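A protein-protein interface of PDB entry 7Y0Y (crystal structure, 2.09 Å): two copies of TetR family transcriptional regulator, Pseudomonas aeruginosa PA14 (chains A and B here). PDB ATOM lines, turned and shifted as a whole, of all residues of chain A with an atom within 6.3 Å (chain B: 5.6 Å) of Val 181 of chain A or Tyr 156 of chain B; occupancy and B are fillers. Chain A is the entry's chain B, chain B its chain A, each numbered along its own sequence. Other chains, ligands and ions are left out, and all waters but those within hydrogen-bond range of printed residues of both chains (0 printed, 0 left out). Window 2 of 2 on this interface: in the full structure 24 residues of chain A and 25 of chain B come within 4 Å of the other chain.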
ATOM      1  N   PRO A 176      -3.251 -30.657  -8.352  1.00  0.00           N
ATOM      2  CA  PRO A 176      -4.542 -31.264  -7.983  1.00  0.00           C
ATOM      3  C   PRO A 176      -5.135 -30.749  -6.675  1.00  0.00           C
ATOM      4  O   PRO A 176      -6.364 -30.814  -6.504  1.00  0.00           O
ATOM      5  CB  PRO A 176      -4.220 -32.767  -7.903  1.00  0.00           C
ATOM      6  CG  PRO A 176      -2.749 -32.912  -8.195  1.00  0.00           C
ATOM      7  CD  PRO A 176      -2.288 -31.650  -8.846  1.00  0.00           C
ATOM      8  N   PHE A 177      -4.319 -30.248  -5.736  1.00  0.00           N
ATOM      9  CA  PHE A 177      -4.898 -29.668  -4.517  1.00  0.00           C
ATOM     10  C   PHE A 177      -5.689 -28.406  -4.849  1.00  0.00           C
ATOM     11  O   PHE A 177      -6.840 -28.249  -4.427  1.00  0.00           O
ATOM     12  CB  PHE A 177      -3.810 -29.359  -3.465  1.00  0.00           C
ATOM     13  CG  PHE A 177      -4.365 -28.873  -2.127  1.00  0.00           C
ATOM     14  CD1 PHE A 177      -4.611 -27.528  -1.914  1.00  0.00           C
ATOM     15  CD2 PHE A 177      -4.660 -29.767  -1.108  1.00  0.00           C
ATOM     16  CE1 PHE A 177      -5.135 -27.084  -0.709  1.00  0.00           C
ATOM     17  CE2 PHE A 177      -5.184 -29.332   0.103  1.00  0.00           C
ATOM     18  CZ  PHE A 177      -5.415 -27.984   0.300  1.00  0.00           C
ATOM     19  N   TRP A 178      -5.073 -27.500  -5.604  1.00  0.00           N
ATOM     20  CA  TRP A 178      -5.728 -26.286  -6.080  1.00  0.00           C
ATOM     21  C   TRP A 178      -7.054 -26.585  -6.764  1.00  0.00           C
ATOM     22  O   TRP A 178      -8.119 -26.102  -6.347  1.00  0.00           O
ATOM     23  CB  TRP A 178      -4.809 -25.582  -7.061  1.00  0.00           C
ATOM     24  CG  TRP A 178      -5.529 -24.559  -7.823  1.00  0.00           C
ATOM     25  CD1 TRP A 178      -6.118 -24.692  -9.052  1.00  0.00           C
ATOM     26  CD2 TRP A 178      -5.776 -23.225  -7.392  1.00  0.00           C
ATOM     27  NE1 TRP A 178      -6.708 -23.502  -9.417  1.00  0.00           N
ATOM     28  CE2 TRP A 178      -6.515 -22.587  -8.411  1.00  0.00           C
ATOM     29  CE3 TRP A 178      -5.450 -22.508  -6.235  1.00  0.00           C
ATOM     30  CZ2 TRP A 178      -6.929 -21.264  -8.307  1.00  0.00           C
ATOM     31  CZ3 TRP A 178      -5.848 -21.198  -6.141  1.00  0.00           C
ATOM     32  CH2 TRP A 178      -6.589 -20.590  -7.162  1.00  0.00           C
ATOM     33  N   ARG A 179      -6.992 -27.377  -7.842  1.00  0.00           N
ATOM     34  CA  ARG A 179      -8.164 -27.665  -8.666  1.00  0.00           C
ATOM     35  C   ARG A 179      -9.333 -28.170  -7.842  1.00  0.00           C
ATOM     36  O   ARG A 179     -10.489 -27.827  -8.112  1.00  0.00           O
ATOM     37  CB  ARG A 179      -7.813 -28.719  -9.713  1.00  0.00           C
ATOM     38  CG  ARG A 179      -7.330 -28.166 -11.023  1.00  0.00           C
ATOM     39  CD  ARG A 179      -7.374 -29.262 -12.084  1.00  0.00           C
ATOM     40  NE  ARG A 179      -6.471 -30.371 -11.792  1.00  0.00           N
ATOM     41  CZ  ARG A 179      -5.148 -30.278 -11.804  1.00  0.00           C
ATOM     42  NH1 ARG A 179      -4.536 -29.126 -12.041  1.00  0.00           N
ATOM     43  NH2 ARG A 179      -4.419 -31.368 -11.573  1.00  0.00           N
ATOM     44  N   GLU A 180      -9.053 -29.002  -6.834  1.00  0.00           N
ATOM     45  CA  GLU A 180     -10.085 -29.845  -6.250  1.00  0.00           C
ATOM     46  C   GLU A 180     -10.386 -29.637  -4.785  1.00  0.00           C
ATOM     47  O   GLU A 180     -11.500 -29.979  -4.363  1.00  0.00           O
ATOM     48  CB  GLU A 180      -9.746 -31.323  -6.420  1.00  0.00           C
ATOM     49  CG  GLU A 180      -9.667 -31.698  -7.837  1.00  0.00           C
ATOM     50  CD  GLU A 180     -11.025 -32.016  -8.267  1.00  0.00           C
ATOM     51  OE1 GLU A 180     -11.540 -33.056  -7.872  1.00  0.00           O
ATOM     52  OE2 GLU A 180     -11.591 -31.247  -9.049  1.00  0.00           O
ATOM     53  N   VAL A 181      -9.449 -29.126  -3.996  1.00  0.00           N
ATOM     54  CA  VAL A 181      -9.671 -28.913  -2.572  1.00  0.00           C
ATOM     55  C   VAL A 181      -9.902 -27.438  -2.255  1.00  0.00           C
ATOM     56  O   VAL A 181     -10.874 -27.093  -1.579  1.00  0.00           O
ATOM     57  CB  VAL A 181      -8.502 -29.506  -1.750  1.00  0.00           C
ATOM     58  CG1 VAL A 181      -8.770 -29.353  -0.264  1.00  0.00           C
ATOM     59  CG2 VAL A 181      -8.341 -30.990  -2.076  1.00  0.00           C
ATOM     60  N   LEU A 182      -9.045 -26.549  -2.763  1.00  0.00           N
ATOM     61  CA  LEU A 182      -9.116 -25.139  -2.383  1.00  0.00           C
ATOM     62  C   LEU A 182     -10.355 -24.475  -2.983  1.00  0.00           C
ATOM     63  O   LEU A 182     -10.529 -24.446  -4.209  1.00  0.00           O
ATOM     64  CB  LEU A 182      -7.855 -24.401  -2.815  1.00  0.00           C
ATOM     65  CG  LEU A 182      -7.889 -22.930  -2.389  1.00  0.00           C
ATOM     66  CD1 LEU A 182      -7.781 -22.828  -0.854  1.00  0.00           C
ATOM     67  CD2 LEU A 182      -6.781 -22.143  -3.055  1.00  0.00           C
ATOM     68  N   GLU A 183     -11.195 -23.916  -2.109  1.00  0.00           N
ATOM     69  CA  GLU A 183     -12.486 -23.334  -2.474  1.00  0.00           C
ATOM     70  C   GLU A 183     -12.384 -21.939  -3.079  1.00  0.00           C
ATOM     71  O   GLU A 183     -12.382 -21.773  -4.304  1.00  0.00           O
ATOM     72  CB  GLU A 183     -13.383 -23.243  -1.249  1.00  0.00           C
ATOM     73  CG  GLU A 183     -13.689 -24.537  -0.592  1.00  0.00           C
ATOM     74  CD  GLU A 183     -14.896 -24.403   0.288  1.00  0.00           C
ATOM     75  OE1 GLU A 183     -16.013 -24.243  -0.253  1.00  0.00           O
ATOM     76  OE2 GLU A 183     -14.721 -24.401   1.522  1.00  0.00           O
ATOM     77  N   PHE A 188      -8.194 -16.271  -2.452  1.00  0.00           N
ATOM     78  CA  PHE A 188      -6.804 -16.681  -2.306  1.00  0.00           C
ATOM     79  C   PHE A 188      -5.880 -15.820  -3.145  1.00  0.00           C
ATOM     80  O   PHE A 188      -4.771 -15.475  -2.712  1.00  0.00           O
ATOM     81  CB  PHE A 188      -6.624 -18.145  -2.703  1.00  0.00           C
ATOM     82  CG  PHE A 188      -5.204 -18.584  -2.642  1.00  0.00           C
ATOM     83  CD1 PHE A 188      -4.588 -18.777  -1.411  1.00  0.00           C
ATOM     84  CD2 PHE A 188      -4.461 -18.749  -3.802  1.00  0.00           C
ATOM     85  CE1 PHE A 188      -3.257 -19.144  -1.346  1.00  0.00           C
ATOM     86  CE2 PHE A 188      -3.148 -19.123  -3.742  1.00  0.00           C
ATOM     87  CZ  PHE A 188      -2.544 -19.332  -2.502  1.00  0.00           C
ATOM     88  N   PHE B 134      -0.588 -33.379   6.643  1.00  0.00           N
ATOM     89  CA  PHE B 134      -1.455 -32.286   6.222  1.00  0.00           C
ATOM     90  C   PHE B 134      -2.238 -31.722   7.407  1.00  0.00           C
ATOM     91  O   PHE B 134      -2.269 -30.504   7.627  1.00  0.00           O
ATOM     92  CB  PHE B 134      -2.397 -32.769   5.117  1.00  0.00           C
ATOM     93  CG  PHE B 134      -3.355 -31.707   4.652  1.00  0.00           C
ATOM     94  CD1 PHE B 134      -2.904 -30.645   3.878  1.00  0.00           C
ATOM     95  CD2 PHE B 134      -4.695 -31.766   5.000  1.00  0.00           C
ATOM     96  CE1 PHE B 134      -3.784 -29.639   3.450  1.00  0.00           C
ATOM     97  CE2 PHE B 134      -5.591 -30.779   4.575  1.00  0.00           C
ATOM     98  CZ  PHE B 134      -5.128 -29.709   3.796  1.00  0.00           C
ATOM     99  N   THR B 138      -1.768 -27.920   9.052  1.00  0.00           N
ATOM    100  CA  THR B 138      -2.946 -27.078   9.167  1.00  0.00           C
ATOM    101  C   THR B 138      -3.285 -26.780  10.620  1.00  0.00           C
ATOM    102  O   THR B 138      -3.778 -25.684  10.934  1.00  0.00           O
ATOM    103  CB  THR B 138      -4.108 -27.776   8.447  1.00  0.00           C
ATOM    104  OG1 THR B 138      -3.770 -27.884   7.058  1.00  0.00           O
ATOM    105  CG2 THR B 138      -5.351 -26.971   8.566  1.00  0.00           C
ATOM    106  N   PRO B 154      -9.003 -18.553   5.670  1.00  0.00           N
ATOM    107  CA  PRO B 154      -9.060 -20.010   5.698  1.00  0.00           C
ATOM    108  C   PRO B 154      -7.671 -20.608   5.861  1.00  0.00           C
ATOM    109  O   PRO B 154      -6.679 -20.093   5.319  1.00  0.00           O
ATOM    110  CB  PRO B 154      -9.686 -20.373   4.346  1.00  0.00           C
ATOM    111  CG  PRO B 154     -10.485 -19.185   3.991  1.00  0.00           C
ATOM    112  CD  PRO B 154      -9.704 -18.013   4.485  1.00  0.00           C
ATOM    113  N   PRO B 155      -7.544 -21.639   6.693  1.00  0.00           N
ATOM    114  CA  PRO B 155      -6.222 -22.220   6.915  1.00  0.00           C
ATOM    115  C   PRO B 155      -5.592 -22.729   5.637  1.00  0.00           C
ATOM    116  O   PRO B 155      -4.362 -22.688   5.503  1.00  0.00           O
ATOM    117  CB  PRO B 155      -6.511 -23.338   7.920  1.00  0.00           C
ATOM    118  CG  PRO B 155      -7.660 -22.802   8.707  1.00  0.00           C
ATOM    119  CD  PRO B 155      -8.532 -22.134   7.662  1.00  0.00           C
ATOM    120  N   TYR B 156      -6.405 -23.159   4.676  1.00  0.00           N
ATOM    121  CA  TYR B 156      -5.875 -23.642   3.406  1.00  0.00           C
ATOM    122  C   TYR B 156      -5.228 -22.524   2.593  1.00  0.00           C
ATOM    123  O   TYR B 156      -4.368 -22.811   1.747  1.00  0.00           O
ATOM    124  CB  TYR B 156      -6.985 -24.330   2.599  1.00  0.00           C
ATOM    125  CG  TYR B 156      -7.524 -25.639   3.193  1.00  0.00           C
ATOM    126  CD1 TYR B 156      -7.148 -26.082   4.467  1.00  0.00           C
ATOM    127  CD2 TYR B 156      -8.429 -26.429   2.480  1.00  0.00           C
ATOM    128  CE1 TYR B 156      -7.659 -27.274   5.009  1.00  0.00           C
ATOM    129  CE2 TYR B 156      -8.940 -27.637   3.017  1.00  0.00           C
ATOM    130  CZ  TYR B 156      -8.549 -28.051   4.277  1.00  0.00           C
ATOM    131  OH  TYR B 156      -9.066 -29.229   4.821  1.00  0.00           O
ATOM    132  N   PHE B 157      -5.585 -21.254   2.841  1.00  0.00           N
ATOM    133  CA  PHE B 157      -4.826 -20.159   2.226  1.00  0.00           C
ATOM    134  C   PHE B 157      -3.366 -20.188   2.667  1.00  0.00           C
ATOM    135  O   PHE B 157      -2.441 -20.086   1.845  1.00  0.00           O
ATOM    136  CB  PHE B 157      -5.417 -18.789   2.593  1.00  0.00           C
ATOM    137  CG  PHE B 157      -6.671 -18.412   1.838  1.00  0.00           C
ATOM    138  CD1 PHE B 157      -7.494 -19.374   1.270  1.00  0.00           C
ATOM    139  CD2 PHE B 157      -7.047 -17.077   1.747  1.00  0.00           C
ATOM    140  CE1 PHE B 157      -8.655 -19.010   0.604  1.00  0.00           C
ATOM    141  CE2 PHE B 157      -8.209 -16.704   1.095  1.00  0.00           C
ATOM    142  CZ  PHE B 157      -9.016 -17.672   0.517  1.00  0.00           C
ATOM    143  N   HIS B 158      -3.137 -20.254   3.972  1.00  0.00           N
ATOM    144  CA  HIS B 158      -1.767 -20.290   4.465  1.00  0.00           C
ATOM    145  C   HIS B 158      -1.059 -21.551   3.992  1.00  0.00           C
ATOM    146  O   HIS B 158       0.123 -21.514   3.643  1.00  0.00           O
ATOM    147  CB  HIS B 158      -1.752 -20.227   5.991  1.00  0.00           C
ATOM    148  CG  HIS B 158      -2.339 -18.970   6.562  1.00  0.00           C
ATOM    149  ND1 HIS B 158      -1.644 -17.779   6.599  1.00  0.00           N
ATOM    150  CD2 HIS B 158      -3.530 -18.727   7.164  1.00  0.00           C
ATOM    151  CE1 HIS B 158      -2.389 -16.852   7.180  1.00  0.00           C
ATOM    152  NE2 HIS B 158      -3.535 -17.399   7.537  1.00  0.00           N
ATOM    153  N   TYR B 159      -1.760 -22.685   4.005  1.00  0.00           N
ATOM    154  CA  TYR B 159      -1.151 -23.930   3.548  1.00  0.00           C
ATOM    155  C   TYR B 159      -0.654 -23.791   2.115  1.00  0.00           C
ATOM    156  O   TYR B 159       0.477 -24.178   1.789  1.00  0.00           O
ATOM    157  CB  TYR B 159      -2.149 -25.083   3.646  1.00  0.00           C
ATOM    158  CG  TYR B 159      -1.609 -26.357   3.033  1.00  0.00           C
ATOM    159  CD1 TYR B 159      -0.785 -27.205   3.769  1.00  0.00           C
ATOM    160  CD2 TYR B 159      -1.863 -26.682   1.709  1.00  0.00           C
ATOM    161  CE1 TYR B 159      -0.263 -28.359   3.210  1.00  0.00           C
ATOM    162  CE2 TYR B 159      -1.349 -27.849   1.143  1.00  0.00           C
ATOM    163  CZ  TYR B 159      -0.554 -28.675   1.904  1.00  0.00           C
ATOM    164  OH  TYR B 159      -0.039 -29.824   1.355  1.00  0.00           O
ATOM    165  N   CYS B 160      -1.491 -23.231   1.243  1.00  0.00           N
ATOM    166  CA  CYS B 160      -1.126 -23.094  -0.161  1.00  0.00           C
ATOM    167  C   CYS B 160      -0.015 -22.071  -0.340  1.00  0.00           C
ATOM    168  O   CYS B 160       0.865 -22.253  -1.182  1.00  0.00           O
ATOM    169  CB  CYS B 160      -2.347 -22.698  -0.988  1.00  0.00           C
ATOM    170  SG  CYS B 160      -3.545 -24.011  -1.153  1.00  0.00           S
ATOM    171  N   ALA B 161      -0.029 -20.991   0.441  1.00  0.00           N
ATOM    172  CA  ALA B 161       1.075 -20.041   0.345  1.00  0.00           C
ATOM    173  C   ALA B 161       2.390 -20.714   0.714  1.00  0.00           C
ATOM    174  O   ALA B 161       3.412 -20.535   0.030  1.00  0.00           O
ATOM    175  CB  ALA B 161       0.818 -18.823   1.244  1.00  0.00           C
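N of Leu 182 of chain A sits at hydrogen-bond distance from O of Phe 177 of chain A, 3.2 Å away. OG1 of Thr 138 of chain B is in hydrogen-bond range of O of Phe 134 of chain B. O of Tyr 156 of chain B sits at hydrogen-bond distance from SG of Cys 160 of chain B (3.2 Å).
Among the printed residues, pairs that only touch across the chains: Phe 177 of chain A with Phe 134 of chain B (3.6 Å), Phe 177 of chain A with Cys 160 of chain B (3.5 Å), Val 181 of chain A with Tyr 156 of chain B (3.7 Å), Leu 182 of chain A with Tyr 156 of chain B (3.8 Å), Phe 188 of chain A with Phe 157 of chain B (3.4 Å) and Phe 188 of chain A with Cys 160 of chain B (3.7 Å).
Val 181 of chain A touches just one residue of chain B: Tyr 156. Tyr 156 of chain B touches two residues of chain A. Of the printed residues of chain B, Leu 182 of chain A touches Tyr 156 (3.8 Å). Printed residues of chain A within 4 Å of Phe 157 of chain B: Phe 188. Pro 155 of chain B touches none of the printed residues of chain A. Ala 161 of chain B touches none of the printed residues of chain A. The nearest residue of chain B that does not touch Val 181 of chain A is Phe 134 of chain B (5.5 Å). The nearest residue of chain A that does not touch Tyr 156 of chain B is Phe 177 of chain A (4.03 Å).
Hydrophobic or aromatic side chains of chain A within 4 Å of the printed part of chain B: Phe 177, Val 181, Leu 182 and Phe 188. Among the printed residues, 6 pairs touch across the chains.
No position is printed for both chains. Of the 6 pairs that touch across the chains among the printed residues, none has its exchanged pair printed and touching as well.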
